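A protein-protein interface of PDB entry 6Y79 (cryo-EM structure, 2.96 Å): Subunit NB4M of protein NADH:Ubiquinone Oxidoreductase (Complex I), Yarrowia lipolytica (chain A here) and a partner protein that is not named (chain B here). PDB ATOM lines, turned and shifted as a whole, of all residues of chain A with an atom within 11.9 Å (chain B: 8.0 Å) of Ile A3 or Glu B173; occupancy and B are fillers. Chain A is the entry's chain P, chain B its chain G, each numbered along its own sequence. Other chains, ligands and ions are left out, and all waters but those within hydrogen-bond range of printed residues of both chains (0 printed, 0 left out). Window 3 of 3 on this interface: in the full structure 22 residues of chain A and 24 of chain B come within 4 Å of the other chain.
Ala A2 touches Asn B176 (CB to ND2, 3.6 Å).
Trp B177 touches Ala A2 (NE1 to CB, 3.7 Å).
CG1 of Ile A3 touches OE1 of Glu B173, at 3.95 Å.
CB of Ala A5 touches OD2 of Asp B195, at 3.2 Å.
Ala A9 touches Asp B195 (CB to OD2, 3.4 Å).
Ala A2 touches just these residues of chain B: Asn B176 and Trp B177.
Printed residues of chain B within 4 Å of Ile A3: Glu B173 (3.95 Å).
Printed residues of chain B within 4 Å of Ala A5: Asp B195 (3.2 Å).
Of the printed residues of chain B, Thr A6 touches Asp B195 (2.6 Å).
Of the printed residues of chain B, Ala A9 touches Asp B195.
Printed residues of chain B within 4 Å of Gln A84: Asp B195 (2.6 Å).
Lys B121 touches none of the printed residues of chain A.
No residue of chain A comes within 4 Å of Thr B169.
No residue of chain A comes within 4 Å of Cys B170.
Glu B173 touches one residue of chain A.
No residue of chain A comes within 4 Å of Gly B174.
Of chain A, only Ala A2 (3.6 Å) comes within 4 Å of Asn B176.
Of the printed residues of chain A, Trp B177 touches Ala A2 (3.7 Å).
The nearest residue of chain B that does not touch Ile A3 is Pro B194 (5.6 Å).
The nearest printed residue of chain A that does not touch Asp B195 is Glu A10 (4.1 Å).
O of Glu B173 sits close to OD1 of Asn B176, at 3.3 Å.
Printed residues of chain A that touch a printed residue of chain B: Ala A2, Ile A3, Ala A5, Thr A6, Ala A9 and Gln A84.
Hydrophobic or aromatic side chains of chain A within 4 Å of the printed part of chain B: Ala A2, Ile A3, Ala A5 and Ala A9.
Hydrophobic or aromatic side chains of chain B within 4 Å of the printed part of chain A: Trp B177.
Along chain B the printed residues that touch a printed residue of chain A span positions 173 to 195.
Among the printed residues, 7 pairs touch across the chains.
Among the printed residues, no Asp or Glu carboxylate lies within 4 Å of a Lys or Arg side-chain nitrogen of the other chain.
The side-chain carboxylate (OD2) of Asp B195 lies within hydrogen-bond range of the backbone NH (N) of Thr A6.
The side-chain amide nitrogen (NE2) of Gln A84 lies within hydrogen-bond range of the side-chain carboxylate (OD1) of Asp B195 (2.6 Å).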
ATOM      1  N   ALA A   2      -8.956   8.663   0.254  1.00  0.00           N
ATOM      2  CA  ALA A   2      -8.693   8.258  -1.113  1.00  0.00           C
ATOM      3  C   ALA A   2      -7.464   7.344  -1.191  1.00  0.00           C
ATOM      4  O   ALA A   2      -6.440   7.732  -1.741  1.00  0.00           O
ATOM      5  CB  ALA A   2      -8.484   9.486  -2.001  1.00  0.00           C
ATOM      6  N   ILE A   3      -7.575   6.144  -0.618  1.00  0.00           N
ATOM      7  CA  ILE A   3      -6.424   5.231  -0.573  1.00  0.00           C
ATOM      8  C   ILE A   3      -6.303   4.459  -1.884  1.00  0.00           C
ATOM      9  O   ILE A   3      -5.207   4.260  -2.415  1.00  0.00           O
ATOM     10  CB  ILE A   3      -6.504   4.260   0.620  1.00  0.00           C
ATOM     11  CG1 ILE A   3      -6.584   5.014   1.946  1.00  0.00           C
ATOM     12  CG2 ILE A   3      -5.283   3.424   0.739  1.00  0.00           C
ATOM     13  CD1 ILE A   3      -7.928   5.131   2.507  1.00  0.00           C
ATOM     14  N   ILE A   4      -7.410   3.971  -2.393  1.00  0.00           N
ATOM     15  CA  ILE A   4      -7.470   3.473  -3.764  1.00  0.00           C
ATOM     16  C   ILE A   4      -7.371   4.683  -4.674  1.00  0.00           C
ATOM     17  O   ILE A   4      -7.936   5.739  -4.392  1.00  0.00           O
ATOM     18  CB  ILE A   4      -8.761   2.659  -4.017  1.00  0.00           C
ATOM     19  CG1 ILE A   4      -8.880   1.509  -3.025  1.00  0.00           C
ATOM     20  CG2 ILE A   4      -8.757   2.047  -5.408  1.00  0.00           C
ATOM     21  CD1 ILE A   4      -7.776   0.472  -3.148  1.00  0.00           C
ATOM     22  N   ALA A   5      -6.611   4.539  -5.750  1.00  0.00           N
ATOM     23  CA  ALA A   5      -6.399   5.580  -6.732  1.00  0.00           C
ATOM     24  C   ALA A   5      -7.144   5.229  -8.019  1.00  0.00           C
ATOM     25  O   ALA A   5      -7.739   4.159  -8.148  1.00  0.00           O
ATOM     26  CB  ALA A   5      -4.902   5.755  -6.961  1.00  0.00           C
ATOM     27  N   THR A   6      -7.096   6.139  -8.987  1.00  0.00           N
ATOM     28  CA  THR A   6      -7.777   5.968 -10.267  1.00  0.00           C
ATOM     29  C   THR A   6      -7.078   4.859 -11.082  1.00  0.00           C
ATOM     30  O   THR A   6      -5.996   4.396 -10.719  1.00  0.00           O
ATOM     31  CB  THR A   6      -7.826   7.345 -10.970  1.00  0.00           C
ATOM     32  OG1 THR A   6      -8.372   8.303 -10.054  1.00  0.00           O
ATOM     33  CG2 THR A   6      -8.702   7.388 -12.194  1.00  0.00           C
ATOM     34  N   ALA A   7      -7.748   4.383 -12.144  1.00  0.00           N
ATOM     35  CA  ALA A   7      -7.280   3.253 -12.939  1.00  0.00           C
ATOM     36  C   ALA A   7      -5.927   3.525 -13.583  1.00  0.00           C
ATOM     37  O   ALA A   7      -4.956   2.798 -13.344  1.00  0.00           O
ATOM     38  CB  ALA A   7      -8.318   2.919 -14.010  1.00  0.00           C
ATOM     39  N   ALA A   9      -3.598   5.608 -13.129  1.00  0.00           N
ATOM     40  CA  ALA A   9      -2.795   6.405 -12.223  1.00  0.00           C
ATOM     41  C   ALA A   9      -1.325   6.038 -12.338  1.00  0.00           C
ATOM     42  O   ALA A   9      -0.959   4.947 -12.779  1.00  0.00           O
ATOM     43  CB  ALA A   9      -3.249   6.196 -10.792  1.00  0.00           C
ATOM     44  N   GLU A  10      -0.478   6.962 -11.898  1.00  0.00           N
ATOM     45  CA  GLU A  10       0.907   6.655 -11.586  1.00  0.00           C
ATOM     46  C   GLU A  10       1.316   7.533 -10.420  1.00  0.00           C
ATOM     47  O   GLU A  10       1.041   8.736 -10.428  1.00  0.00           O
ATOM     48  CB  GLU A  10       1.828   6.888 -12.776  1.00  0.00           C
ATOM     49  CG  GLU A  10       3.252   6.508 -12.478  1.00  0.00           C
ATOM     50  CD  GLU A  10       4.131   6.557 -13.692  1.00  0.00           C
ATOM     51  OE1 GLU A  10       3.629   6.913 -14.775  1.00  0.00           O
ATOM     52  OE2 GLU A  10       5.327   6.238 -13.560  1.00  0.00           O
ATOM     53  N   THR A  11       1.898   6.907  -9.399  1.00  0.00           N
ATOM     54  CA  THR A  11       2.569   7.632  -8.332  1.00  0.00           C
ATOM     55  C   THR A  11       3.647   8.506  -8.934  1.00  0.00           C
ATOM     56  O   THR A  11       4.527   8.008  -9.641  1.00  0.00           O
ATOM     57  CB  THR A  11       3.181   6.659  -7.331  1.00  0.00           C
ATOM     58  OG1 THR A  11       2.146   5.881  -6.717  1.00  0.00           O
ATOM     59  CG2 THR A  11       3.944   7.411  -6.264  1.00  0.00           C
ATOM     60  N   GLN A  84      -3.977  10.498 -18.684  1.00  0.00           N
ATOM     61  CA  GLN A  84      -4.975   9.983 -17.751  1.00  0.00           C
ATOM     62  C   GLN A  84      -6.321  10.677 -17.928  1.00  0.00           C
ATOM     63  O   GLN A  84      -7.373  10.046 -17.789  1.00  0.00           O
ATOM     64  CB  GLN A  84      -4.475  10.144 -16.319  1.00  0.00           C
ATOM     65  CG  GLN A  84      -5.365   9.526 -15.269  1.00  0.00           C
ATOM     66  CD  GLN A  84      -4.929   9.871 -13.872  1.00  0.00           C
ATOM     67  OE1 GLN A  84      -3.955  10.592 -13.676  1.00  0.00           O
ATOM     68  NE2 GLN A  84      -5.655   9.370 -12.887  1.00  0.00           N
ATOM     69  N   LYS B 121      -2.433  15.412  15.151  1.00  0.00           N
ATOM     70  CA  LYS B 121      -3.092  14.345  14.412  1.00  0.00           C
ATOM     71  C   LYS B 121      -3.760  14.870  13.157  1.00  0.00           C
ATOM     72  O   LYS B 121      -3.618  14.286  12.079  1.00  0.00           O
ATOM     73  CB  LYS B 121      -4.126  13.656  15.297  1.00  0.00           C
ATOM     74  CG  LYS B 121      -3.539  12.802  16.380  1.00  0.00           C
ATOM     75  CD  LYS B 121      -2.669  11.732  15.785  1.00  0.00           C
ATOM     76  CE  LYS B 121      -1.861  11.054  16.850  1.00  0.00           C
ATOM     77  NZ  LYS B 121      -1.155   9.887  16.285  1.00  0.00           N
ATOM     78  N   ILE B 123      -4.578  16.932   9.987  1.00  0.00           N
ATOM     79  CA  ILE B 123      -4.214  17.870   8.941  1.00  0.00           C
ATOM     80  C   ILE B 123      -5.361  18.856   8.764  1.00  0.00           C
ATOM     81  O   ILE B 123      -6.539  18.495   8.873  1.00  0.00           O
ATOM     82  CB  ILE B 123      -3.874  17.109   7.646  1.00  0.00           C
ATOM     83  CG1 ILE B 123      -3.303  18.040   6.596  1.00  0.00           C
ATOM     84  CG2 ILE B 123      -5.032  16.280   7.131  1.00  0.00           C
ATOM     85  CD1 ILE B 123      -1.964  18.451   6.972  1.00  0.00           C
ATOM     86  N   ILE B 168       3.217  14.317   2.096  1.00  0.00           N
ATOM     87  CA  ILE B 168       2.898  13.744   3.391  1.00  0.00           C
ATOM     88  C   ILE B 168       1.626  12.903   3.333  1.00  0.00           C
ATOM     89  O   ILE B 168       1.104  12.507   4.369  1.00  0.00           O
ATOM     90  CB  ILE B 168       2.806  14.812   4.488  1.00  0.00           C
ATOM     91  CG1 ILE B 168       1.698  15.813   4.176  1.00  0.00           C
ATOM     92  CG2 ILE B 168       4.129  15.521   4.647  1.00  0.00           C
ATOM     93  CD1 ILE B 168       1.268  16.620   5.367  1.00  0.00           C
ATOM     94  N   THR B 169       1.153  12.570   2.127  1.00  0.00           N
ATOM     95  CA  THR B 169       0.037  11.637   1.997  1.00  0.00           C
ATOM     96  C   THR B 169       0.423  10.219   2.420  1.00  0.00           C
ATOM     97  O   THR B 169      -0.471   9.385   2.601  1.00  0.00           O
ATOM     98  CB  THR B 169      -0.516  11.654   0.568  1.00  0.00           C
ATOM     99  OG1 THR B 169      -1.880  11.228   0.582  1.00  0.00           O
ATOM    100  CG2 THR B 169       0.264  10.727  -0.347  1.00  0.00           C
ATOM    101  N   CYS B 170       1.722   9.933   2.595  1.00  0.00           N
ATOM    102  CA  CYS B 170       2.144   8.716   3.273  1.00  0.00           C
ATOM    103  C   CYS B 170       1.545   8.652   4.682  1.00  0.00           C
ATOM    104  O   CYS B 170       1.084   7.598   5.120  1.00  0.00           O
ATOM    105  CB  CYS B 170       3.670   8.671   3.320  1.00  0.00           C
ATOM    106  SG  CYS B 170       4.483   9.059   1.738  1.00  0.00           S
ATOM    107  N   LEU B 171       1.502   9.781   5.391  1.00  0.00           N
ATOM    108  CA  LEU B 171       1.088   9.784   6.795  1.00  0.00           C
ATOM    109  C   LEU B 171      -0.392  10.102   6.945  1.00  0.00           C
ATOM    110  O   LEU B 171      -1.091   9.491   7.758  1.00  0.00           O
ATOM    111  CB  LEU B 171       1.908  10.807   7.575  1.00  0.00           C
ATOM    112  CG  LEU B 171       3.413  10.607   7.628  1.00  0.00           C
ATOM    113  CD1 LEU B 171       4.058  11.844   8.169  1.00  0.00           C
ATOM    114  CD2 LEU B 171       3.741   9.433   8.506  1.00  0.00           C
ATOM    115  N   TYR B 172      -0.876  11.079   6.192  1.00  0.00           N
ATOM    116  CA  TYR B 172      -2.229  11.595   6.313  1.00  0.00           C
ATOM    117  C   TYR B 172      -3.014  11.238   5.070  1.00  0.00           C
ATOM    118  O   TYR B 172      -2.623  11.609   3.962  1.00  0.00           O
ATOM    119  CB  TYR B 172      -2.201  13.098   6.475  1.00  0.00           C
ATOM    120  CG  TYR B 172      -1.633  13.535   7.776  1.00  0.00           C
ATOM    121  CD1 TYR B 172      -1.883  12.829   8.933  1.00  0.00           C
ATOM    122  CD2 TYR B 172      -0.813  14.631   7.846  1.00  0.00           C
ATOM    123  CE1 TYR B 172      -1.351  13.232  10.131  1.00  0.00           C
ATOM    124  CE2 TYR B 172      -0.280  15.031   9.026  1.00  0.00           C
ATOM    125  CZ  TYR B 172      -0.550  14.341  10.166  1.00  0.00           C
ATOM    126  OH  TYR B 172       0.001  14.770  11.344  1.00  0.00           O
ATOM    127  N   GLU B 173      -4.128  10.541   5.249  1.00  0.00           N
ATOM    128  CA  GLU B 173      -4.910  10.209   4.074  1.00  0.00           C
ATOM    129  C   GLU B 173      -5.780  11.380   3.642  1.00  0.00           C
ATOM    130  O   GLU B 173      -6.218  11.425   2.489  1.00  0.00           O
ATOM    131  CB  GLU B 173      -5.730   8.945   4.329  1.00  0.00           C
ATOM    132  CG  GLU B 173      -4.885   7.667   4.507  1.00  0.00           C
ATOM    133  CD  GLU B 173      -3.620   7.611   3.646  1.00  0.00           C
ATOM    134  OE1 GLU B 173      -3.711   7.694   2.399  1.00  0.00           O
ATOM    135  OE2 GLU B 173      -2.516   7.492   4.222  1.00  0.00           O
ATOM    136  N   GLY B 174      -6.009  12.344   4.525  1.00  0.00           N
ATOM    137  CA  GLY B 174      -6.731  13.537   4.160  1.00  0.00           C
ATOM    138  C   GLY B 174      -5.914  14.610   3.494  1.00  0.00           C
ATOM    139  O   GLY B 174      -6.466  15.622   3.062  1.00  0.00           O
ATOM    140  N   ALA B 175      -4.607  14.413   3.373  1.00  0.00           N
ATOM    141  CA  ALA B 175      -3.729  15.455   2.869  1.00  0.00           C
ATOM    142  C   ALA B 175      -3.754  15.593   1.356  1.00  0.00           C
ATOM    143  O   ALA B 175      -3.569  16.711   0.860  1.00  0.00           O
ATOM    144  CB  ALA B 175      -2.296  15.192   3.321  1.00  0.00           C
ATOM    145  N   ASN B 176      -4.022  14.506   0.619  1.00  0.00           N
ATOM    146  CA  ASN B 176      -3.659  14.459  -0.794  1.00  0.00           C
ATOM    147  C   ASN B 176      -4.468  15.415  -1.655  1.00  0.00           C
ATOM    148  O   ASN B 176      -3.874  16.093  -2.504  1.00  0.00           O
ATOM    149  CB  ASN B 176      -3.770  13.035  -1.346  1.00  0.00           C
ATOM    150  CG  ASN B 176      -5.123  12.429  -1.164  1.00  0.00           C
ATOM    151  OD1 ASN B 176      -5.961  12.961  -0.450  1.00  0.00           O
ATOM    152  ND2 ASN B 176      -5.353  11.302  -1.824  1.00  0.00           N
ATOM    153  N   TRP B 177      -5.785  15.513  -1.410  1.00  0.00           N
ATOM    154  CA  TRP B 177      -6.630  16.495  -2.089  1.00  0.00           C
ATOM    155  C   TRP B 177      -6.090  17.898  -1.903  1.00  0.00           C
ATOM    156  O   TRP B 177      -5.966  18.651  -2.878  1.00  0.00           O
ATOM    157  CB  TRP B 177      -8.060  16.422  -1.561  1.00  0.00           C
ATOM    158  CG  TRP B 177      -8.756  15.157  -1.876  1.00  0.00           C
ATOM    159  CD1 TRP B 177      -8.764  14.021  -1.129  1.00  0.00           C
ATOM    160  CD2 TRP B 177      -9.567  14.892  -3.015  1.00  0.00           C
ATOM    161  NE1 TRP B 177      -9.517  13.055  -1.745  1.00  0.00           N
ATOM    162  CE2 TRP B 177     -10.025  13.571  -2.907  1.00  0.00           C
ATOM    163  CE3 TRP B 177      -9.953  15.642  -4.113  1.00  0.00           C
ATOM    164  CZ2 TRP B 177     -10.846  12.989  -3.861  1.00  0.00           C
ATOM    165  CZ3 TRP B 177     -10.765  15.066  -5.060  1.00  0.00           C
ATOM    166  CH2 TRP B 177     -11.204  13.754  -4.931  1.00  0.00           C
ATOM    167  N   PHE B 178      -5.667  18.216  -0.672  1.00  0.00           N
ATOM    168  CA  PHE B 178      -5.053  19.503  -0.380  1.00  0.00           C
ATOM    169  C   PHE B 178      -3.790  19.706  -1.195  1.00  0.00           C
ATOM    170  O   PHE B 178      -3.645  20.745  -1.854  1.00  0.00           O
ATOM    171  CB  PHE B 178      -4.728  19.604   1.099  1.00  0.00           C
ATOM    172  CG  PHE B 178      -5.914  19.775   1.971  1.00  0.00           C
ATOM    173  CD1 PHE B 178      -6.618  20.962   1.981  1.00  0.00           C
ATOM    174  CD2 PHE B 178      -6.304  18.761   2.815  1.00  0.00           C
ATOM    175  CE1 PHE B 178      -7.708  21.118   2.804  1.00  0.00           C
ATOM    176  CE2 PHE B 178      -7.391  18.907   3.636  1.00  0.00           C
ATOM    177  CZ  PHE B 178      -8.094  20.086   3.634  1.00  0.00           C
ATOM    178  N   PRO B 194       0.058   9.419  -5.121  1.00  0.00           N
ATOM    179  CA  PRO B 194      -0.848   8.744  -6.047  1.00  0.00           C
ATOM    180  C   PRO B 194      -1.911   9.697  -6.560  1.00  0.00           C
ATOM    181  O   PRO B 194      -2.632  10.322  -5.774  1.00  0.00           O
ATOM    182  CB  PRO B 194      -1.455   7.630  -5.198  1.00  0.00           C
ATOM    183  CG  PRO B 194      -1.290   8.076  -3.796  1.00  0.00           C
ATOM    184  CD  PRO B 194      -0.057   8.910  -3.749  1.00  0.00           C
ATOM    185  N   ASP B 195      -1.982   9.801  -7.897  1.00  0.00           N
ATOM    186  CA  ASP B 195      -2.946  10.656  -8.597  1.00  0.00           C
ATOM    187  C   ASP B 195      -2.799  12.119  -8.227  1.00  0.00           C
ATOM    188  O   ASP B 195      -3.708  12.748  -7.694  1.00  0.00           O
ATOM    189  CB  ASP B 195      -4.377  10.164  -8.385  1.00  0.00           C
ATOM    190  CG  ASP B 195      -4.793   9.162  -9.436  1.00  0.00           C
ATOM    191  OD1 ASP B 195      -4.427   9.374 -10.607  1.00  0.00           O
ATOM    192  OD2 ASP B 195      -5.397   8.156  -9.056  1.00  0.00           O
